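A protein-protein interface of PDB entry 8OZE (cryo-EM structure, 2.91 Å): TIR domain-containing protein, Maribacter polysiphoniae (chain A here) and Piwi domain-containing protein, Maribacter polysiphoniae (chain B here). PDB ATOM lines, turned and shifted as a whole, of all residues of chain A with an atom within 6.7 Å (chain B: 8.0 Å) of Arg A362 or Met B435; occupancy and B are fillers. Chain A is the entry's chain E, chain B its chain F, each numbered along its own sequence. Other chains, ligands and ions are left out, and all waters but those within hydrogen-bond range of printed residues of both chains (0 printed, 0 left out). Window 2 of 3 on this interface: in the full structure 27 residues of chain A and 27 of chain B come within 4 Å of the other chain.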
ATOM      1  N   GLN A 314      35.944 -14.093  13.876  1.00  0.00           N
ATOM      2  CA  GLN A 314      36.030 -14.130  12.418  1.00  0.00           C
ATOM      3  C   GLN A 314      37.152 -13.172  12.028  1.00  0.00           C
ATOM      4  O   GLN A 314      36.962 -11.952  12.054  1.00  0.00           O
ATOM      5  CB  GLN A 314      34.709 -13.742  11.770  1.00  0.00           C
ATOM      6  CG  GLN A 314      34.715 -13.844  10.255  1.00  0.00           C
ATOM      7  CD  GLN A 314      33.718 -12.909   9.603  1.00  0.00           C
ATOM      8  OE1 GLN A 314      33.669 -11.721   9.916  1.00  0.00           O
ATOM      9  NE2 GLN A 314      32.917 -13.442   8.690  1.00  0.00           N
ATOM     10  N   ILE A 341      23.647  -9.666  13.422  1.00  0.00           N
ATOM     11  CA  ILE A 341      25.027 -10.017  13.730  1.00  0.00           C
ATOM     12  C   ILE A 341      25.836  -8.732  13.797  1.00  0.00           C
ATOM     13  O   ILE A 341      25.781  -7.911  12.874  1.00  0.00           O
ATOM     14  CB  ILE A 341      25.618 -10.978  12.685  1.00  0.00           C
ATOM     15  CG1 ILE A 341      24.695 -12.177  12.478  1.00  0.00           C
ATOM     16  CG2 ILE A 341      26.998 -11.435  13.107  1.00  0.00           C
ATOM     17  CD1 ILE A 341      24.952 -12.916  11.189  1.00  0.00           C
ATOM     18  N   PHE A 343      29.708  -6.749  15.031  1.00  0.00           N
ATOM     19  CA  PHE A 343      31.139  -7.006  15.015  1.00  0.00           C
ATOM     20  C   PHE A 343      31.881  -5.972  15.845  1.00  0.00           C
ATOM     21  O   PHE A 343      31.500  -4.799  15.886  1.00  0.00           O
ATOM     22  CB  PHE A 343      31.668  -7.022  13.584  1.00  0.00           C
ATOM     23  CG  PHE A 343      31.219  -8.214  12.798  1.00  0.00           C
ATOM     24  CD1 PHE A 343      29.967  -8.241  12.214  1.00  0.00           C
ATOM     25  CD2 PHE A 343      32.041  -9.316  12.662  1.00  0.00           C
ATOM     26  CE1 PHE A 343      29.547  -9.339  11.504  1.00  0.00           C
ATOM     27  CE2 PHE A 343      31.627 -10.418  11.946  1.00  0.00           C
ATOM     28  CZ  PHE A 343      30.378 -10.429  11.368  1.00  0.00           C
ATOM     29  N   GLN A 357      30.759  -2.901   9.001  1.00  0.00           N
ATOM     30  CA  GLN A 357      29.841  -3.768   9.731  1.00  0.00           C
ATOM     31  C   GLN A 357      28.901  -4.500   8.783  1.00  0.00           C
ATOM     32  O   GLN A 357      28.626  -5.689   8.972  1.00  0.00           O
ATOM     33  CB  GLN A 357      29.046  -2.955  10.752  1.00  0.00           C
ATOM     34  CG  GLN A 357      29.844  -2.543  11.972  1.00  0.00           C
ATOM     35  CD  GLN A 357      29.609  -3.462  13.153  1.00  0.00           C
ATOM     36  OE1 GLN A 357      29.327  -4.647  12.982  1.00  0.00           O
ATOM     37  NE2 GLN A 357      29.718  -2.919  14.358  1.00  0.00           N
ATOM     38  N   HIS A 358      28.399  -3.809   7.758  1.00  0.00           N
ATOM     39  CA  HIS A 358      27.505  -4.449   6.798  1.00  0.00           C
ATOM     40  C   HIS A 358      28.214  -5.571   6.050  1.00  0.00           C
ATOM     41  O   HIS A 358      27.672  -6.673   5.894  1.00  0.00           O
ATOM     42  CB  HIS A 358      26.964  -3.407   5.818  1.00  0.00           C
ATOM     43  CG  HIS A 358      26.127  -3.987   4.721  1.00  0.00           C
ATOM     44  ND1 HIS A 358      25.304  -5.076   4.908  1.00  0.00           N
ATOM     45  CD2 HIS A 358      25.991  -3.631   3.422  1.00  0.00           C
ATOM     46  CE1 HIS A 358      24.694  -5.363   3.772  1.00  0.00           C
ATOM     47  NE2 HIS A 358      25.094  -4.503   2.855  1.00  0.00           N
ATOM     48  N   SER A 359      29.435  -5.306   5.578  1.00  0.00           N
ATOM     49  CA  SER A 359      30.186  -6.326   4.856  1.00  0.00           C
ATOM     50  C   SER A 359      30.490  -7.518   5.752  1.00  0.00           C
ATOM     51  O   SER A 359      30.353  -8.672   5.329  1.00  0.00           O
ATOM     52  CB  SER A 359      31.477  -5.730   4.297  1.00  0.00           C
ATOM     53  OG  SER A 359      32.392  -5.435   5.337  1.00  0.00           O
ATOM     54  N   SER A 360      30.897  -7.259   6.997  1.00  0.00           N
ATOM     55  CA  SER A 360      31.186  -8.351   7.919  1.00  0.00           C
ATOM     56  C   SER A 360      29.935  -9.164   8.217  1.00  0.00           C
ATOM     57  O   SER A 360      29.993 -10.396   8.297  1.00  0.00           O
ATOM     58  CB  SER A 360      31.791  -7.798   9.208  1.00  0.00           C
ATOM     59  OG  SER A 360      32.931  -7.006   8.929  1.00  0.00           O
ATOM     60  N   ARG A 361      28.796  -8.492   8.391  1.00  0.00           N
ATOM     61  CA  ARG A 361      27.551  -9.204   8.653  1.00  0.00           C
ATOM     62  C   ARG A 361      27.163 -10.082   7.472  1.00  0.00           C
ATOM     63  O   ARG A 361      26.729 -11.225   7.658  1.00  0.00           O
ATOM     64  CB  ARG A 361      26.440  -8.206   8.978  1.00  0.00           C
ATOM     65  CG  ARG A 361      25.169  -8.837   9.514  1.00  0.00           C
ATOM     66  CD  ARG A 361      24.117  -8.956   8.433  1.00  0.00           C
ATOM     67  NE  ARG A 361      22.800  -9.259   8.977  1.00  0.00           N
ATOM     68  CZ  ARG A 361      22.280 -10.476   9.044  1.00  0.00           C
ATOM     69  NH1 ARG A 361      22.941 -11.535   8.610  1.00  0.00           N
ATOM     70  NH2 ARG A 361      21.063 -10.632   9.556  1.00  0.00           N
ATOM     71  N   ARG A 362      27.311  -9.569   6.249  1.00  0.00           N
ATOM     72  CA  ARG A 362      27.026 -10.386   5.073  1.00  0.00           C
ATOM     73  C   ARG A 362      27.961 -11.587   4.996  1.00  0.00           C
ATOM     74  O   ARG A 362      27.522 -12.711   4.718  1.00  0.00           O
ATOM     75  CB  ARG A 362      27.134  -9.538   3.807  1.00  0.00           C
ATOM     76  CG  ARG A 362      26.023  -8.517   3.641  1.00  0.00           C
ATOM     77  CD  ARG A 362      24.795  -9.134   2.988  1.00  0.00           C
ATOM     78  NE  ARG A 362      23.917  -9.781   3.956  1.00  0.00           N
ATOM     79  CZ  ARG A 362      22.983 -10.668   3.645  1.00  0.00           C
ATOM     80  NH1 ARG A 362      22.778 -11.044   2.394  1.00  0.00           N
ATOM     81  NH2 ARG A 362      22.238 -11.194   4.612  1.00  0.00           N
ATOM     82  N   ARG A 363      29.254 -11.370   5.257  1.00  0.00           N
ATOM     83  CA  ARG A 363      30.212 -12.472   5.220  1.00  0.00           C
ATOM     84  C   ARG A 363      29.869 -13.536   6.253  1.00  0.00           C
ATOM     85  O   ARG A 363      29.933 -14.737   5.964  1.00  0.00           O
ATOM     86  CB  ARG A 363      31.630 -11.945   5.448  1.00  0.00           C
ATOM     87  CG  ARG A 363      32.135 -11.018   4.355  1.00  0.00           C
ATOM     88  CD  ARG A 363      32.696 -11.797   3.180  1.00  0.00           C
ATOM     89  NE  ARG A 363      32.985 -10.931   2.043  1.00  0.00           N
ATOM     90  CZ  ARG A 363      34.095 -10.220   1.906  1.00  0.00           C
ATOM     91  NH1 ARG A 363      35.051 -10.245   2.821  1.00  0.00           N
ATOM     92  NH2 ARG A 363      34.250  -9.461   0.824  1.00  0.00           N
ATOM     93  N   GLN A 364      29.500 -13.116   7.463  1.00  0.00           N
ATOM     94  CA  GLN A 364      29.195 -14.080   8.515  1.00  0.00           C
ATOM     95  C   GLN A 364      27.888 -14.811   8.237  1.00  0.00           C
ATOM     96  O   GLN A 364      27.784 -16.017   8.485  1.00  0.00           O
ATOM     97  CB  GLN A 364      29.146 -13.381   9.873  1.00  0.00           C
ATOM     98  CG  GLN A 364      28.671 -14.266  11.014  1.00  0.00           C
ATOM     99  CD  GLN A 364      29.689 -15.325  11.401  1.00  0.00           C
ATOM    100  OE1 GLN A 364      30.386 -15.189  12.402  1.00  0.00           O
ATOM    101  NE2 GLN A 364      29.766 -16.394  10.616  1.00  0.00           N
ATOM    102  N   GLY A 365      26.882 -14.107   7.725  1.00  0.00           N
ATOM    103  CA  GLY A 365      25.621 -14.735   7.405  1.00  0.00           C
ATOM    104  C   GLY A 365      25.615 -15.548   6.135  1.00  0.00           C
ATOM    105  O   GLY A 365      24.636 -16.248   5.865  1.00  0.00           O
ATOM    106  N   LYS A 366      26.684 -15.462   5.340  1.00  0.00           N
ATOM    107  CA  LYS A 366      26.788 -16.288   4.142  1.00  0.00           C
ATOM    108  C   LYS A 366      26.603 -17.771   4.448  1.00  0.00           C
ATOM    109  O   LYS A 366      26.028 -18.501   3.633  1.00  0.00           O
ATOM    110  CB  LYS A 366      28.140 -16.051   3.467  1.00  0.00           C
ATOM    111  CG  LYS A 366      28.336 -16.804   2.164  1.00  0.00           C
ATOM    112  CD  LYS A 366      29.701 -16.511   1.568  1.00  0.00           C
ATOM    113  CE  LYS A 366      29.934 -17.312   0.299  1.00  0.00           C
ATOM    114  NZ  LYS A 366      31.277 -17.041  -0.283  1.00  0.00           N
ATOM    115  N   ASN A 367      27.070 -18.236   5.607  1.00  0.00           N
ATOM    116  CA  ASN A 367      26.996 -19.651   5.953  1.00  0.00           C
ATOM    117  C   ASN A 367      26.128 -19.932   7.175  1.00  0.00           C
ATOM    118  O   ASN A 367      26.304 -20.974   7.816  1.00  0.00           O
ATOM    119  CB  ASN A 367      28.400 -20.222   6.172  1.00  0.00           C
ATOM    120  CG  ASN A 367      29.228 -19.388   7.127  1.00  0.00           C
ATOM    121  OD1 ASN A 367      28.705 -18.535   7.840  1.00  0.00           O
ATOM    122  ND2 ASN A 367      30.534 -19.632   7.145  1.00  0.00           N
ATOM    123  N   TRP A 368      25.203 -19.039   7.520  1.00  0.00           N
ATOM    124  CA  TRP A 368      24.279 -19.265   8.632  1.00  0.00           C
ATOM    125  C   TRP A 368      22.941 -19.725   8.070  1.00  0.00           C
ATOM    126  O   TRP A 368      22.166 -18.925   7.540  1.00  0.00           O
ATOM    127  CB  TRP A 368      24.122 -18.006   9.472  1.00  0.00           C
ATOM    128  CG  TRP A 368      25.257 -17.761  10.399  1.00  0.00           C
ATOM    129  CD1 TRP A 368      26.521 -18.253  10.295  1.00  0.00           C
ATOM    130  CD2 TRP A 368      25.226 -16.981  11.596  1.00  0.00           C
ATOM    131  NE1 TRP A 368      27.287 -17.817  11.347  1.00  0.00           N
ATOM    132  CE2 TRP A 368      26.512 -17.033  12.162  1.00  0.00           C
ATOM    133  CE3 TRP A 368      24.235 -16.237  12.243  1.00  0.00           C
ATOM    134  CZ2 TRP A 368      26.835 -16.371  13.341  1.00  0.00           C
ATOM    135  CZ3 TRP A 368      24.557 -15.582  13.413  1.00  0.00           C
ATOM    136  CH2 TRP A 368      25.846 -15.651  13.949  1.00  0.00           C
ATOM    137  N   TRP A 369      22.665 -21.016   8.194  1.00  0.00           N
ATOM    138  CA  TRP A 369      21.456 -21.614   7.648  1.00  0.00           C
ATOM    139  C   TRP A 369      20.365 -21.644   8.721  1.00  0.00           C
ATOM    140  O   TRP A 369      20.466 -20.966   9.746  1.00  0.00           O
ATOM    141  CB  TRP A 369      21.792 -22.987   7.062  1.00  0.00           C
ATOM    142  CG  TRP A 369      22.934 -22.925   6.091  1.00  0.00           C
ATOM    143  CD1 TRP A 369      24.124 -23.582   6.183  1.00  0.00           C
ATOM    144  CD2 TRP A 369      22.996 -22.148   4.887  1.00  0.00           C
ATOM    145  NE1 TRP A 369      24.923 -23.269   5.109  1.00  0.00           N
ATOM    146  CE2 TRP A 369      24.253 -22.391   4.299  1.00  0.00           C
ATOM    147  CE3 TRP A 369      22.109 -21.276   4.247  1.00  0.00           C
ATOM    148  CZ2 TRP A 369      24.644 -21.793   3.103  1.00  0.00           C
ATOM    149  CZ3 TRP A 369      22.500 -20.683   3.061  1.00  0.00           C
ATOM    150  CH2 TRP A 369      23.756 -20.944   2.502  1.00  0.00           C
ATOM    151  N   TRP A 373      20.471 -19.874  12.737  1.00  0.00           N
ATOM    152  CA  TRP A 373      19.704 -18.718  13.181  1.00  0.00           C
ATOM    153  C   TRP A 373      18.715 -19.090  14.276  1.00  0.00           C
ATOM    154  O   TRP A 373      18.611 -18.389  15.288  1.00  0.00           O
ATOM    155  CB  TRP A 373      18.949 -18.097  12.001  1.00  0.00           C
ATOM    156  CG  TRP A 373      19.811 -17.330  11.064  1.00  0.00           C
ATOM    157  CD1 TRP A 373      20.340 -17.776   9.892  1.00  0.00           C
ATOM    158  CD2 TRP A 373      20.239 -15.974  11.209  1.00  0.00           C
ATOM    159  NE1 TRP A 373      21.077 -16.783   9.300  1.00  0.00           N
ATOM    160  CE2 TRP A 373      21.032 -15.666  10.089  1.00  0.00           C
ATOM    161  CE3 TRP A 373      20.031 -14.990  12.179  1.00  0.00           C
ATOM    162  CZ2 TRP A 373      21.615 -14.417   9.911  1.00  0.00           C
ATOM    163  CZ3 TRP A 373      20.612 -13.751  12.000  1.00  0.00           C
ATOM    164  CH2 TRP A 373      21.395 -13.476  10.875  1.00  0.00           C
ATOM    165  N   ASP B 402      18.829 -27.779   8.081  1.00  0.00           N
ATOM    166  CA  ASP B 402      19.355 -26.492   7.647  1.00  0.00           C
ATOM    167  C   ASP B 402      18.672 -26.021   6.369  1.00  0.00           C
ATOM    168  O   ASP B 402      19.341 -25.711   5.379  1.00  0.00           O
ATOM    169  CB  ASP B 402      20.869 -26.573   7.432  1.00  0.00           C
ATOM    170  CG  ASP B 402      21.635 -26.670   8.734  1.00  0.00           C
ATOM    171  OD1 ASP B 402      21.148 -26.137   9.752  1.00  0.00           O
ATOM    172  OD2 ASP B 402      22.728 -27.276   8.740  1.00  0.00           O
ATOM    173  N   THR B 404      14.875 -23.797   4.930  1.00  0.00           N
ATOM    174  CA  THR B 404      13.803 -22.897   5.322  1.00  0.00           C
ATOM    175  C   THR B 404      12.447 -23.518   4.989  1.00  0.00           C
ATOM    176  O   THR B 404      12.347 -24.681   4.590  1.00  0.00           O
ATOM    177  CB  THR B 404      13.985 -21.537   4.652  1.00  0.00           C
ATOM    178  OG1 THR B 404      14.038 -21.703   3.231  1.00  0.00           O
ATOM    179  CG2 THR B 404      15.270 -20.882   5.127  1.00  0.00           C
ATOM    180  N   VAL B 423       8.500 -16.601  -1.271  1.00  0.00           N
ATOM    181  CA  VAL B 423       9.912 -16.957  -1.275  1.00  0.00           C
ATOM    182  C   VAL B 423      10.095 -18.076  -0.261  1.00  0.00           C
ATOM    183  O   VAL B 423       9.860 -17.886   0.937  1.00  0.00           O
ATOM    184  CB  VAL B 423      10.803 -15.758  -0.939  1.00  0.00           C
ATOM    185  CG1 VAL B 423      12.256 -16.142  -1.073  1.00  0.00           C
ATOM    186  CG2 VAL B 423      10.476 -14.586  -1.831  1.00  0.00           C
ATOM    187  N   THR B 431      16.344 -26.336  -3.815  1.00  0.00           N
ATOM    188  CA  THR B 431      16.682 -25.506  -2.667  1.00  0.00           C
ATOM    189  C   THR B 431      15.565 -24.488  -2.464  1.00  0.00           C
ATOM    190  O   THR B 431      14.474 -24.617  -3.029  1.00  0.00           O
ATOM    191  CB  THR B 431      18.051 -24.841  -2.867  1.00  0.00           C
ATOM    192  OG1 THR B 431      18.390 -24.074  -1.704  1.00  0.00           O
ATOM    193  CG2 THR B 431      18.035 -23.932  -4.088  1.00  0.00           C
ATOM    194  N   ALA B 432      15.828 -23.484  -1.636  1.00  0.00           N
ATOM    195  CA  ALA B 432      14.892 -22.392  -1.434  1.00  0.00           C
ATOM    196  C   ALA B 432      15.297 -21.196  -2.285  1.00  0.00           C
ATOM    197  O   ALA B 432      16.477 -20.990  -2.580  1.00  0.00           O
ATOM    198  CB  ALA B 432      14.832 -21.991   0.041  1.00  0.00           C
ATOM    199  N   LEU B 433      14.299 -20.406  -2.682  1.00  0.00           N
ATOM    200  CA  LEU B 433      14.552 -19.253  -3.538  1.00  0.00           C
ATOM    201  C   LEU B 433      15.328 -18.148  -2.833  1.00  0.00           C
ATOM    202  O   LEU B 433      15.891 -17.283  -3.512  1.00  0.00           O
ATOM    203  CB  LEU B 433      13.233 -18.695  -4.073  1.00  0.00           C
ATOM    204  CG  LEU B 433      12.617 -19.399  -5.285  1.00  0.00           C
ATOM    205  CD1 LEU B 433      11.877 -20.659  -4.877  1.00  0.00           C
ATOM    206  CD2 LEU B 433      11.689 -18.453  -6.021  1.00  0.00           C
ATOM    207  N   SER B 434      15.377 -18.154  -1.504  1.00  0.00           N
ATOM    208  CA  SER B 434      16.101 -17.140  -0.758  1.00  0.00           C
ATOM    209  C   SER B 434      17.498 -17.639  -0.397  1.00  0.00           C
ATOM    210  O   SER B 434      17.947 -18.700  -0.834  1.00  0.00           O
ATOM    211  CB  SER B 434      15.329 -16.749   0.500  1.00  0.00           C
ATOM    212  OG  SER B 434      15.058 -17.886   1.299  1.00  0.00           O
ATOM    213  N   MET B 435      18.196 -16.852   0.417  1.00  0.00           N
ATOM    214  CA  MET B 435      19.490 -17.230   0.965  1.00  0.00           C
ATOM    215  C   MET B 435      19.432 -17.412   2.472  1.00  0.00           C
ATOM    216  O   MET B 435      19.813 -18.473   2.981  1.00  0.00           O
ATOM    217  CB  MET B 435      20.544 -16.176   0.592  1.00  0.00           C
ATOM    218  CG  MET B 435      21.981 -16.640   0.744  1.00  0.00           C
ATOM    219  SD  MET B 435      22.727 -16.112   2.294  1.00  0.00           S
ATOM    220  CE  MET B 435      23.052 -14.387   1.946  1.00  0.00           C
ATOM    221  N   GLU B 436      18.961 -16.406   3.200  1.00  0.00           N
ATOM    222  CA  GLU B 436      18.670 -16.535   4.618  1.00  0.00           C
ATOM    223  C   GLU B 436      17.204 -16.928   4.786  1.00  0.00           C
ATOM    224  O   GLU B 436      16.529 -17.310   3.826  1.00  0.00           O
ATOM    225  CB  GLU B 436      19.013 -15.238   5.348  1.00  0.00           C
ATOM    226  CG  GLU B 436      20.486 -14.893   5.294  1.00  0.00           C
ATOM    227  CD  GLU B 436      21.349 -15.960   5.931  1.00  0.00           C
ATOM    228  OE1 GLU B 436      21.434 -15.991   7.174  1.00  0.00           O
ATOM    229  OE2 GLU B 436      21.933 -16.780   5.194  1.00  0.00           O
ATOM    230  N   VAL B 437      16.692 -16.847   6.010  1.00  0.00           N
ATOM    231  CA  VAL B 437      15.290 -17.161   6.264  1.00  0.00           C
ATOM    232  C   VAL B 437      14.431 -16.069   5.638  1.00  0.00           C
ATOM    233  O   VAL B 437      14.565 -14.891   6.000  1.00  0.00           O
ATOM    234  CB  VAL B 437      15.014 -17.306   7.767  1.00  0.00           C
ATOM    235  CG1 VAL B 437      13.581 -17.752   7.998  1.00  0.00           C
ATOM    236  CG2 VAL B 437      15.991 -18.295   8.380  1.00  0.00           C
ATOM    237  N   PRO B 438      13.543 -16.408   4.711  1.00  0.00           N
ATOM    238  CA  PRO B 438      12.822 -15.381   3.957  1.00  0.00           C
ATOM    239  C   PRO B 438      11.722 -14.722   4.774  1.00  0.00           C
ATOM    240  O   PRO B 438      11.233 -15.256   5.771  1.00  0.00           O
ATOM    241  CB  PRO B 438      12.231 -16.167   2.785  1.00  0.00           C
ATOM    242  CG  PRO B 438      12.014 -17.527   3.347  1.00  0.00           C
ATOM    243  CD  PRO B 438      13.161 -17.768   4.294  1.00  0.00           C
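O of Gly A365 lies close to OE2 of Glu B436.
OE1 of Glu B436 lies close to O of Trp A368 (3.0 Å).
OE1 of Glu B436 sits close to NE1 of Trp A373 (2.3 Å).
The side-chain amide nitrogen of Gln A364 sits close to the indole nitrogen of Trp A368, 3.0 Å away.
OG of Ser B434 is in hydrogen-bond range of O of Glu B436 (3.0 Å).
The backbone carbonyl oxygen of Trp A368 is in hydrogen-bond range of the indole nitrogen of Trp A373 (3.0 Å).
Among the printed residues, pairs that only touch across the chains: Arg A362 with Met B435 (3.4 Å), Trp A369 with Met B435 (3.5 Å) and Trp A369 with Asp B402 (3.7 Å).
Of chain B, only Met B435 (3.4 Å) comes within 4 Å of Arg A362.
Met B435 touches two residues of chain A.
Of the printed residues of chain B, Trp A368 touches Glu B436.
Of the printed residues of chain B, Trp A373 touches Glu B436.
The nearest residue of chain A that does not touch Met B435 is Gly A365 (4.1 Å).
Printed residues of chain A that touch a printed residue of chain B: Arg A362, Gly A365, Trp A368, Trp A369 and Trp A373.
Hydrophobic or aromatic side chains of chain A within 4 Å of the printed part of chain B: Trp A369 and Trp A373.
Of the 11 printed residues of chain B, 3 touch a printed residue of chain A.
Printed residues of chain B that touch a printed residue of chain A: Asp B402, Met B435 and Glu B436.
Hydrophobic or aromatic side chains of chain B that line the printed part of chain A: Met B435.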
